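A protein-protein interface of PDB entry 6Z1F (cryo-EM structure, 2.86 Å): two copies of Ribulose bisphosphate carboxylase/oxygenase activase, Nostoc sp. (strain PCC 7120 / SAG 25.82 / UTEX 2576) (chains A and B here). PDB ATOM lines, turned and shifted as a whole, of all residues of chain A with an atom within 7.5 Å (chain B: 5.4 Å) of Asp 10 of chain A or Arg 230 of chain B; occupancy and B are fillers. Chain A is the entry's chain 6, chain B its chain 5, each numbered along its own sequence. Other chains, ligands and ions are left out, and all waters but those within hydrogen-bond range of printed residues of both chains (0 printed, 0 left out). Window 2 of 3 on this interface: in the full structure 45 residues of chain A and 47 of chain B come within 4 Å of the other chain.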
ATOM      1  N   ALA A   5     -14.845 -27.991  18.869  1.00  0.00           N
ATOM      2  CA  ALA A   5     -13.741 -27.967  19.811  1.00  0.00           C
ATOM      3  C   ALA A   5     -12.701 -26.958  19.330  1.00  0.00           C
ATOM      4  O   ALA A   5     -12.292 -27.005  18.171  1.00  0.00           O
ATOM      5  CB  ALA A   5     -13.159 -29.350  19.968  1.00  0.00           C
ATOM      6  N   PRO A   6     -12.276 -25.995  20.186  1.00  0.00           N
ATOM      7  CA  PRO A   6     -11.310 -24.966  19.786  1.00  0.00           C
ATOM      8  C   PRO A   6      -9.972 -25.494  19.268  1.00  0.00           C
ATOM      9  O   PRO A   6      -9.336 -24.840  18.442  1.00  0.00           O
ATOM     10  CB  PRO A   6     -11.124 -24.144  21.071  1.00  0.00           C
ATOM     11  CG  PRO A   6     -12.414 -24.360  21.824  1.00  0.00           C
ATOM     12  CD  PRO A   6     -12.734 -25.817  21.572  1.00  0.00           C
ATOM     13  N   ARG A   7      -9.566 -26.676  19.750  1.00  0.00           N
ATOM     14  CA  ARG A   7      -8.344 -27.333  19.310  1.00  0.00           C
ATOM     15  C   ARG A   7      -8.477 -27.752  17.848  1.00  0.00           C
ATOM     16  O   ARG A   7      -7.537 -27.593  17.072  1.00  0.00           O
ATOM     17  CB  ARG A   7      -8.050 -28.577  20.155  1.00  0.00           C
ATOM     18  CG  ARG A   7      -7.695 -28.295  21.608  1.00  0.00           C
ATOM     19  CD  ARG A   7      -7.079 -29.519  22.258  1.00  0.00           C
ATOM     20  NE  ARG A   7      -7.975 -30.668  22.252  1.00  0.00           N
ATOM     21  CZ  ARG A   7      -7.592 -31.937  22.335  1.00  0.00           C
ATOM     22  NH1 ARG A   7      -8.499 -32.900  22.318  1.00  0.00           N
ATOM     23  NH2 ARG A   7      -6.311 -32.248  22.434  1.00  0.00           N
ATOM     24  N   PHE A   8      -9.657 -28.280  17.502  1.00  0.00           N
ATOM     25  CA  PHE A   8      -9.951 -28.827  16.188  1.00  0.00           C
ATOM     26  C   PHE A   8     -10.002 -27.714  15.143  1.00  0.00           C
ATOM     27  O   PHE A   8      -9.482 -27.885  14.042  1.00  0.00           O
ATOM     28  CB  PHE A   8     -11.274 -29.594  16.229  1.00  0.00           C
ATOM     29  CG  PHE A   8     -11.426 -30.657  15.176  1.00  0.00           C
ATOM     30  CD1 PHE A   8     -11.728 -30.323  13.862  1.00  0.00           C
ATOM     31  CD2 PHE A   8     -11.286 -31.996  15.508  1.00  0.00           C
ATOM     32  CE1 PHE A   8     -11.866 -31.308  12.895  1.00  0.00           C
ATOM     33  CE2 PHE A   8     -11.431 -32.982  14.543  1.00  0.00           C
ATOM     34  CZ  PHE A   8     -11.718 -32.636  13.239  1.00  0.00           C
ATOM     35  N   LEU A   9     -10.627 -26.584  15.502  1.00  0.00           N
ATOM     36  CA  LEU A   9     -10.864 -25.493  14.569  1.00  0.00           C
ATOM     37  C   LEU A   9      -9.554 -24.776  14.246  1.00  0.00           C
ATOM     38  O   LEU A   9      -9.359 -24.344  13.113  1.00  0.00           O
ATOM     39  CB  LEU A   9     -11.908 -24.532  15.151  1.00  0.00           C
ATOM     40  CG  LEU A   9     -12.301 -23.347  14.265  1.00  0.00           C
ATOM     41  CD1 LEU A   9     -13.123 -23.789  13.062  1.00  0.00           C
ATOM     42  CD2 LEU A   9     -13.049 -22.294  15.067  1.00  0.00           C
ATOM     43  N   ASP A  10      -8.668 -24.674  15.242  1.00  0.00           N
ATOM     44  CA  ASP A  10      -7.411 -23.955  15.102  1.00  0.00           C
ATOM     45  C   ASP A  10      -6.422 -24.746  14.250  1.00  0.00           C
ATOM     46  O   ASP A  10      -5.600 -24.152  13.557  1.00  0.00           O
ATOM     47  CB  ASP A  10      -6.837 -23.563  16.465  1.00  0.00           C
ATOM     48  CG  ASP A  10      -7.601 -22.437  17.148  1.00  0.00           C
ATOM     49  OD1 ASP A  10      -8.830 -22.326  16.921  1.00  0.00           O
ATOM     50  OD2 ASP A  10      -6.963 -21.674  17.904  1.00  0.00           O
ATOM     51  N   LYS A  11      -6.516 -26.081  14.302  1.00  0.00           N
ATOM     52  CA  LYS A  11      -5.653 -26.960  13.530  1.00  0.00           C
ATOM     53  C   LYS A  11      -6.018 -26.887  12.048  1.00  0.00           C
ATOM     54  O   LYS A  11      -5.127 -26.872  11.203  1.00  0.00           O
ATOM     55  CB  LYS A  11      -5.721 -28.399  14.058  1.00  0.00           C
ATOM     56  CG  LYS A  11      -4.514 -29.275  13.740  1.00  0.00           C
ATOM     57  CD  LYS A  11      -3.342 -29.055  14.677  1.00  0.00           C
ATOM     58  CE  LYS A  11      -2.022 -29.541  14.116  1.00  0.00           C
ATOM     59  NZ  LYS A  11      -1.867 -31.007  14.264  1.00  0.00           N
ATOM     60  N   LEU A  12      -7.324 -26.837  11.750  1.00  0.00           N
ATOM     61  CA  LEU A  12      -7.820 -26.744  10.384  1.00  0.00           C
ATOM     62  C   LEU A  12      -7.483 -25.382   9.779  1.00  0.00           C
ATOM     63  O   LEU A  12      -6.931 -25.321   8.682  1.00  0.00           O
ATOM     64  CB  LEU A  12      -9.330 -27.005  10.356  1.00  0.00           C
ATOM     65  CG  LEU A  12      -9.759 -28.443  10.055  1.00  0.00           C
ATOM     66  CD1 LEU A  12     -11.245 -28.632  10.331  1.00  0.00           C
ATOM     67  CD2 LEU A  12      -9.437 -28.834   8.617  1.00  0.00           C
ATOM     68  N   ALA A  13      -7.811 -24.306  10.512  1.00  0.00           N
ATOM     69  CA  ALA A  13      -7.699 -22.934  10.037  1.00  0.00           C
ATOM     70  C   ALA A  13      -6.257 -22.592   9.671  1.00  0.00           C
ATOM     71  O   ALA A  13      -6.013 -22.050   8.594  1.00  0.00           O
ATOM     72  CB  ALA A  13      -8.244 -21.978  11.068  1.00  0.00           C
ATOM     73  N   VAL A  14      -5.322 -22.937  10.568  1.00  0.00           N
ATOM     74  CA  VAL A  14      -3.910 -22.616  10.417  1.00  0.00           C
ATOM     75  C   VAL A  14      -3.309 -23.404   9.251  1.00  0.00           C
ATOM     76  O   VAL A  14      -2.408 -22.902   8.580  1.00  0.00           O
ATOM     77  CB  VAL A  14      -3.142 -22.800  11.742  1.00  0.00           C
ATOM     78  CG1 VAL A  14      -1.628 -22.793  11.572  1.00  0.00           C
ATOM     79  CG2 VAL A  14      -3.554 -21.745  12.759  1.00  0.00           C
ATOM     80  N   HIS A  15      -3.829 -24.614   8.999  1.00  0.00           N
ATOM     81  CA  HIS A  15      -3.367 -25.438   7.892  1.00  0.00           C
ATOM     82  C   HIS A  15      -3.754 -24.825   6.547  1.00  0.00           C
ATOM     83  O   HIS A  15      -2.909 -24.729   5.656  1.00  0.00           O
ATOM     84  CB  HIS A  15      -3.846 -26.889   8.021  1.00  0.00           C
ATOM     85  CG  HIS A  15      -3.505 -27.722   6.830  1.00  0.00           C
ATOM     86  ND1 HIS A  15      -2.249 -28.268   6.647  1.00  0.00           N
ATOM     87  CD2 HIS A  15      -4.238 -28.081   5.751  1.00  0.00           C
ATOM     88  CE1 HIS A  15      -2.226 -28.937   5.511  1.00  0.00           C
ATOM     89  NE2 HIS A  15      -3.437 -28.838   4.944  1.00  0.00           N
ATOM     90  N   ILE A  16      -5.027 -24.421   6.410  1.00  0.00           N
ATOM     91  CA  ILE A  16      -5.540 -23.910   5.145  1.00  0.00           C
ATOM     92  C   ILE A  16      -4.930 -22.537   4.854  1.00  0.00           C
ATOM     93  O   ILE A  16      -4.468 -22.300   3.739  1.00  0.00           O
ATOM     94  CB  ILE A  16      -7.083 -23.924   5.077  1.00  0.00           C
ATOM     95  CG1 ILE A  16      -7.653 -25.311   5.382  1.00  0.00           C
ATOM     96  CG2 ILE A  16      -7.566 -23.428   3.721  1.00  0.00           C
ATOM     97  CD1 ILE A  16      -9.164 -25.358   5.481  1.00  0.00           C
ATOM     98  N   THR A  17      -4.900 -21.656   5.865  1.00  0.00           N
ATOM     99  CA  THR A  17      -4.418 -20.292   5.700  1.00  0.00           C
ATOM    100  C   THR A  17      -2.961 -20.288   5.238  1.00  0.00           C
ATOM    101  O   THR A  17      -2.603 -19.539   4.328  1.00  0.00           O
ATOM    102  CB  THR A  17      -4.643 -19.452   6.965  1.00  0.00           C
ATOM    103  OG1 THR A  17      -5.972 -19.699   7.428  1.00  0.00           O
ATOM    104  CG2 THR A  17      -4.460 -17.967   6.736  1.00  0.00           C
ATOM    105  N   MET A  53     -16.317 -20.675   7.919  1.00  0.00           N
ATOM    106  CA  MET A  53     -15.427 -19.886   7.079  1.00  0.00           C
ATOM    107  C   MET A  53     -16.073 -19.627   5.718  1.00  0.00           C
ATOM    108  O   MET A  53     -15.657 -18.718   5.003  1.00  0.00           O
ATOM    109  CB  MET A  53     -14.086 -20.596   6.878  1.00  0.00           C
ATOM    110  CG  MET A  53     -13.307 -20.793   8.165  1.00  0.00           C
ATOM    111  SD  MET A  53     -11.624 -21.391   7.869  1.00  0.00           S
ATOM    112  CE  MET A  53     -11.416 -22.478   9.278  1.00  0.00           C
ATOM    113  N   TYR B 225       5.959 -20.745  12.813  1.00  0.00           N
ATOM    114  CA  TYR B 225       5.185 -19.638  12.271  1.00  0.00           C
ATOM    115  C   TYR B 225       3.714 -19.704  12.684  1.00  0.00           C
ATOM    116  O   TYR B 225       2.953 -18.791  12.364  1.00  0.00           O
ATOM    117  CB  TYR B 225       5.329 -19.584  10.748  1.00  0.00           C
ATOM    118  CG  TYR B 225       6.433 -18.685  10.256  1.00  0.00           C
ATOM    119  CD1 TYR B 225       7.728 -19.160  10.098  1.00  0.00           C
ATOM    120  CD2 TYR B 225       6.184 -17.355   9.947  1.00  0.00           C
ATOM    121  CE1 TYR B 225       8.750 -18.337   9.649  1.00  0.00           C
ATOM    122  CE2 TYR B 225       7.194 -16.519   9.496  1.00  0.00           C
ATOM    123  CZ  TYR B 225       8.482 -17.012   9.347  1.00  0.00           C
ATOM    124  OH  TYR B 225       9.482 -16.195   8.903  1.00  0.00           O
ATOM    125  N   ASP B 226       3.329 -20.762  13.412  1.00  0.00           N
ATOM    126  CA  ASP B 226       1.939 -21.075  13.711  1.00  0.00           C
ATOM    127  C   ASP B 226       1.285 -19.999  14.578  1.00  0.00           C
ATOM    128  O   ASP B 226       0.146 -19.613  14.313  1.00  0.00           O
ATOM    129  CB  ASP B 226       1.797 -22.462  14.345  1.00  0.00           C
ATOM    130  CG  ASP B 226       1.892 -23.608  13.351  1.00  0.00           C
ATOM    131  OD1 ASP B 226       1.680 -23.364  12.149  1.00  0.00           O
ATOM    132  OD2 ASP B 226       2.168 -24.743  13.789  1.00  0.00           O
ATOM    133  N   ILE B 227       2.013 -19.530  15.602  1.00  0.00           N
ATOM    134  CA  ILE B 227       1.480 -18.636  16.621  1.00  0.00           C
ATOM    135  C   ILE B 227       1.030 -17.328  15.973  1.00  0.00           C
ATOM    136  O   ILE B 227      -0.071 -16.851  16.246  1.00  0.00           O
ATOM    137  CB  ILE B 227       2.494 -18.410  17.767  1.00  0.00           C
ATOM    138  CG1 ILE B 227       3.157 -19.707  18.246  1.00  0.00           C
ATOM    139  CG2 ILE B 227       1.870 -17.627  18.917  1.00  0.00           C
ATOM    140  CD1 ILE B 227       2.216 -20.740  18.848  1.00  0.00           C
ATOM    141  N   GLN B 228       1.889 -16.779  15.104  1.00  0.00           N
ATOM    142  CA  GLN B 228       1.638 -15.529  14.406  1.00  0.00           C
ATOM    143  C   GLN B 228       0.405 -15.663  13.516  1.00  0.00           C
ATOM    144  O   GLN B 228      -0.418 -14.750  13.471  1.00  0.00           O
ATOM    145  CB  GLN B 228       2.861 -15.117  13.582  1.00  0.00           C
ATOM    146  CG  GLN B 228       4.039 -14.642  14.419  1.00  0.00           C
ATOM    147  CD  GLN B 228       5.141 -14.069  13.561  1.00  0.00           C
ATOM    148  OE1 GLN B 228       5.658 -14.720  12.656  1.00  0.00           O
ATOM    149  NE2 GLN B 228       5.516 -12.835  13.850  1.00  0.00           N
ATOM    150  N   ILE B 229       0.291 -16.809  12.831  1.00  0.00           N
ATOM    151  CA  ILE B 229      -0.767 -17.061  11.864  1.00  0.00           C
ATOM    152  C   ILE B 229      -2.097 -17.234  12.596  1.00  0.00           C
ATOM    153  O   ILE B 229      -3.117 -16.726  12.136  1.00  0.00           O
ATOM    154  CB  ILE B 229      -0.412 -18.242  10.931  1.00  0.00           C
ATOM    155  CG1 ILE B 229       0.654 -17.835   9.910  1.00  0.00           C
ATOM    156  CG2 ILE B 229      -1.647 -18.813  10.241  1.00  0.00           C
ATOM    157  CD1 ILE B 229       1.453 -18.991   9.347  1.00  0.00           C
ATOM    158  N   ARG B 230      -2.064 -17.921  13.744  1.00  0.00           N
ATOM    159  CA  ARG B 230      -3.252 -18.157  14.553  1.00  0.00           C
ATOM    160  C   ARG B 230      -3.825 -16.833  15.065  1.00  0.00           C
ATOM    161  O   ARG B 230      -5.043 -16.660  15.096  1.00  0.00           O
ATOM    162  CB  ARG B 230      -2.932 -19.118  15.702  1.00  0.00           C
ATOM    163  CG  ARG B 230      -4.160 -19.697  16.391  1.00  0.00           C
ATOM    164  CD  ARG B 230      -3.843 -20.404  17.697  1.00  0.00           C
ATOM    165  NE  ARG B 230      -3.298 -19.498  18.703  1.00  0.00           N
ATOM    166  CZ  ARG B 230      -4.012 -18.709  19.504  1.00  0.00           C
ATOM    167  NH1 ARG B 230      -3.393 -17.928  20.374  1.00  0.00           N
ATOM    168  NH2 ARG B 230      -5.332 -18.696  19.440  1.00  0.00           N
ATOM    169  N   ASP B 231      -2.929 -15.913  15.457  1.00  0.00           N
ATOM    170  CA  ASP B 231      -3.277 -14.597  15.975  1.00  0.00           C
ATOM    171  C   ASP B 231      -3.940 -13.758  14.887  1.00  0.00           C
ATOM    172  O   ASP B 231      -4.888 -13.024  15.162  1.00  0.00           O
ATOM    173  CB  ASP B 231      -2.048 -13.882  16.545  1.00  0.00           C
ATOM    174  CG  ASP B 231      -1.553 -14.434  17.874  1.00  0.00           C
ATOM    175  OD1 ASP B 231      -2.065 -15.488  18.310  1.00  0.00           O
ATOM    176  OD2 ASP B 231      -0.655 -13.802  18.468  1.00  0.00           O
ATOM    177  N   PHE B 232      -3.426 -13.887  13.658  1.00  0.00           N
ATOM    178  CA  PHE B 232      -3.896 -13.135  12.508  1.00  0.00           C
ATOM    179  C   PHE B 232      -5.328 -13.530  12.154  1.00  0.00           C
ATOM    180  O   PHE B 232      -6.107 -12.679  11.731  1.00  0.00           O
ATOM    181  CB  PHE B 232      -2.944 -13.320  11.324  1.00  0.00           C
ATOM    182  CG  PHE B 232      -3.473 -12.827  10.001  1.00  0.00           C
ATOM    183  CD1 PHE B 232      -3.401 -11.481   9.666  1.00  0.00           C
ATOM    184  CD2 PHE B 232      -4.044 -13.710   9.093  1.00  0.00           C
ATOM    185  CE1 PHE B 232      -3.891 -11.029   8.449  1.00  0.00           C
ATOM    186  CE2 PHE B 232      -4.533 -13.257   7.875  1.00  0.00           C
ATOM    187  CZ  PHE B 232      -4.453 -11.917   7.556  1.00  0.00           C
ATOM    188  N   ILE B 233      -5.655 -14.819  12.318  1.00  0.00           N
ATOM    189  CA  ILE B 233      -6.963 -15.349  11.953  1.00  0.00           C
ATOM    190  C   ILE B 233      -8.014 -14.821  12.930  1.00  0.00           C
ATOM    191  O   ILE B 233      -9.133 -14.510  12.519  1.00  0.00           O
ATOM    192  CB  ILE B 233      -6.946 -16.892  11.822  1.00  0.00           C
ATOM    193  CG1 ILE B 233      -6.041 -17.341  10.669  1.00  0.00           C
ATOM    194  CG2 ILE B 233      -8.352 -17.460  11.660  1.00  0.00           C
ATOM    195  CD1 ILE B 233      -5.515 -18.754  10.788  1.00  0.00           C
ATOM    196  N   HIS B 234      -7.632 -14.682  14.207  1.00  0.00           N
ATOM    197  CA  HIS B 234      -8.508 -14.170  15.252  1.00  0.00           C
ATOM    198  C   HIS B 234      -8.796 -12.679  15.062  1.00  0.00           C
ATOM    199  O   HIS B 234      -9.936 -12.247  15.235  1.00  0.00           O
ATOM    200  CB  HIS B 234      -7.925 -14.476  16.638  1.00  0.00           C
ATOM    201  CG  HIS B 234      -8.315 -15.813  17.174  1.00  0.00           C
ATOM    202  ND1 HIS B 234      -8.812 -15.976  18.452  1.00  0.00           N
ATOM    203  CD2 HIS B 234      -8.290 -17.044  16.616  1.00  0.00           C
ATOM    204  CE1 HIS B 234      -9.070 -17.252  18.661  1.00  0.00           C
ATOM    205  NE2 HIS B 234      -8.761 -17.929  17.548  1.00  0.00           N
ATOM    206  N   PHE B 238     -12.977 -15.271  11.982  1.00  0.00           N
ATOM    207  CA  PHE B 238     -13.172 -16.540  11.296  1.00  0.00           C
ATOM    208  C   PHE B 238     -14.198 -16.421  10.172  1.00  0.00           C
ATOM    209  O   PHE B 238     -14.160 -17.201   9.220  1.00  0.00           O
ATOM    210  CB  PHE B 238     -13.616 -17.618  12.288  1.00  0.00           C
ATOM    211  CG  PHE B 238     -12.487 -18.360  12.955  1.00  0.00           C
ATOM    212  CD1 PHE B 238     -11.912 -19.468  12.346  1.00  0.00           C
ATOM    213  CD2 PHE B 238     -11.999 -17.952  14.190  1.00  0.00           C
ATOM    214  CE1 PHE B 238     -10.869 -20.151  12.957  1.00  0.00           C
ATOM    215  CE2 PHE B 238     -10.958 -18.638  14.802  1.00  0.00           C
ATOM    216  CZ  PHE B 238     -10.396 -19.736  14.184  1.00  0.00           C
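No position is printed for both chains. Of the 8 pairs that touch across the chains among the printed residues, none has its exchanged pair printed and touching as well.
The guanidinium group of Arg 230 of chain B lies within salt-bridge range of the side-chain carboxylate of Asp 10 of chain A (3.7 Å).
Of the printed residues of chain B, Leu 9 of chain A touches Phe 238. Of chain B, only Arg 230 (3.4 Å) comes within 4 Å of Asp 10 of chain A. Printed residues of chain B within 4 Å of Thr 17 of chain A: Ile 233 (3.5 Å). Of the printed residues of chain B, Met 53 of chain A touches Phe 238 (3.7 Å). Ile 227 of chain B touches none of the printed residues of chain A. Of the printed residues of chain A, Arg 230 of chain B touches Asp 10 and Val 14. Printed residues of chain A within 4 Å of Ile 233 of chain B: Ala 13 and Thr 17. The nearest residue of chain B that does not touch Asp 10 of chain A is Phe 238 of chain B (4.1 Å).
Along chain A the printed residues that touch a printed residue of chain B span positions 9 to 53. Of the 11 printed residues of chain B, 4 touch a printed residue of chain A. Printed residues of chain B that touch a printed residue of chain A: Asp 226, Arg 230, Ile 233 and Phe 238. Hydrophobic or aromatic side chains of chain B that line the printed part of chain A: Ile 233 and Phe 238. Along chain B the printed residues that touch a printed residue of chain A span positions 226 to 238.
Leu 9 of chain A touches Phe 238 of chain B. Ile 233 of chain B touches Ala 13 of chain A. CB of Ala 13 of chain A touches CE1 of Phe 238 of chain B, at 3.7 Å. Asp 226 of chain B touches Val 14 of chain A (OD1 to CG1, 3.4 Å). Val 14 of chain A touches Arg 230 of chain B (CG2 to CB, 3.99 Å). Ile 233 of chain B touches Thr 17 of chain A. Met 53 of chain A touches Phe 238 of chain B (CA to O, 3.7 Å).
NH1 of Arg 230 of chain B is in salt-bridge range of OD1 of Asp 231 of chain B (3.5 Å). The backbone carbonyl oxygen (O) of Ala 13 of chain A sits at hydrogen-bond distance from the side-chain hydroxyl (OG1) of Thr 17 of chain A, at 2.6 Å.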
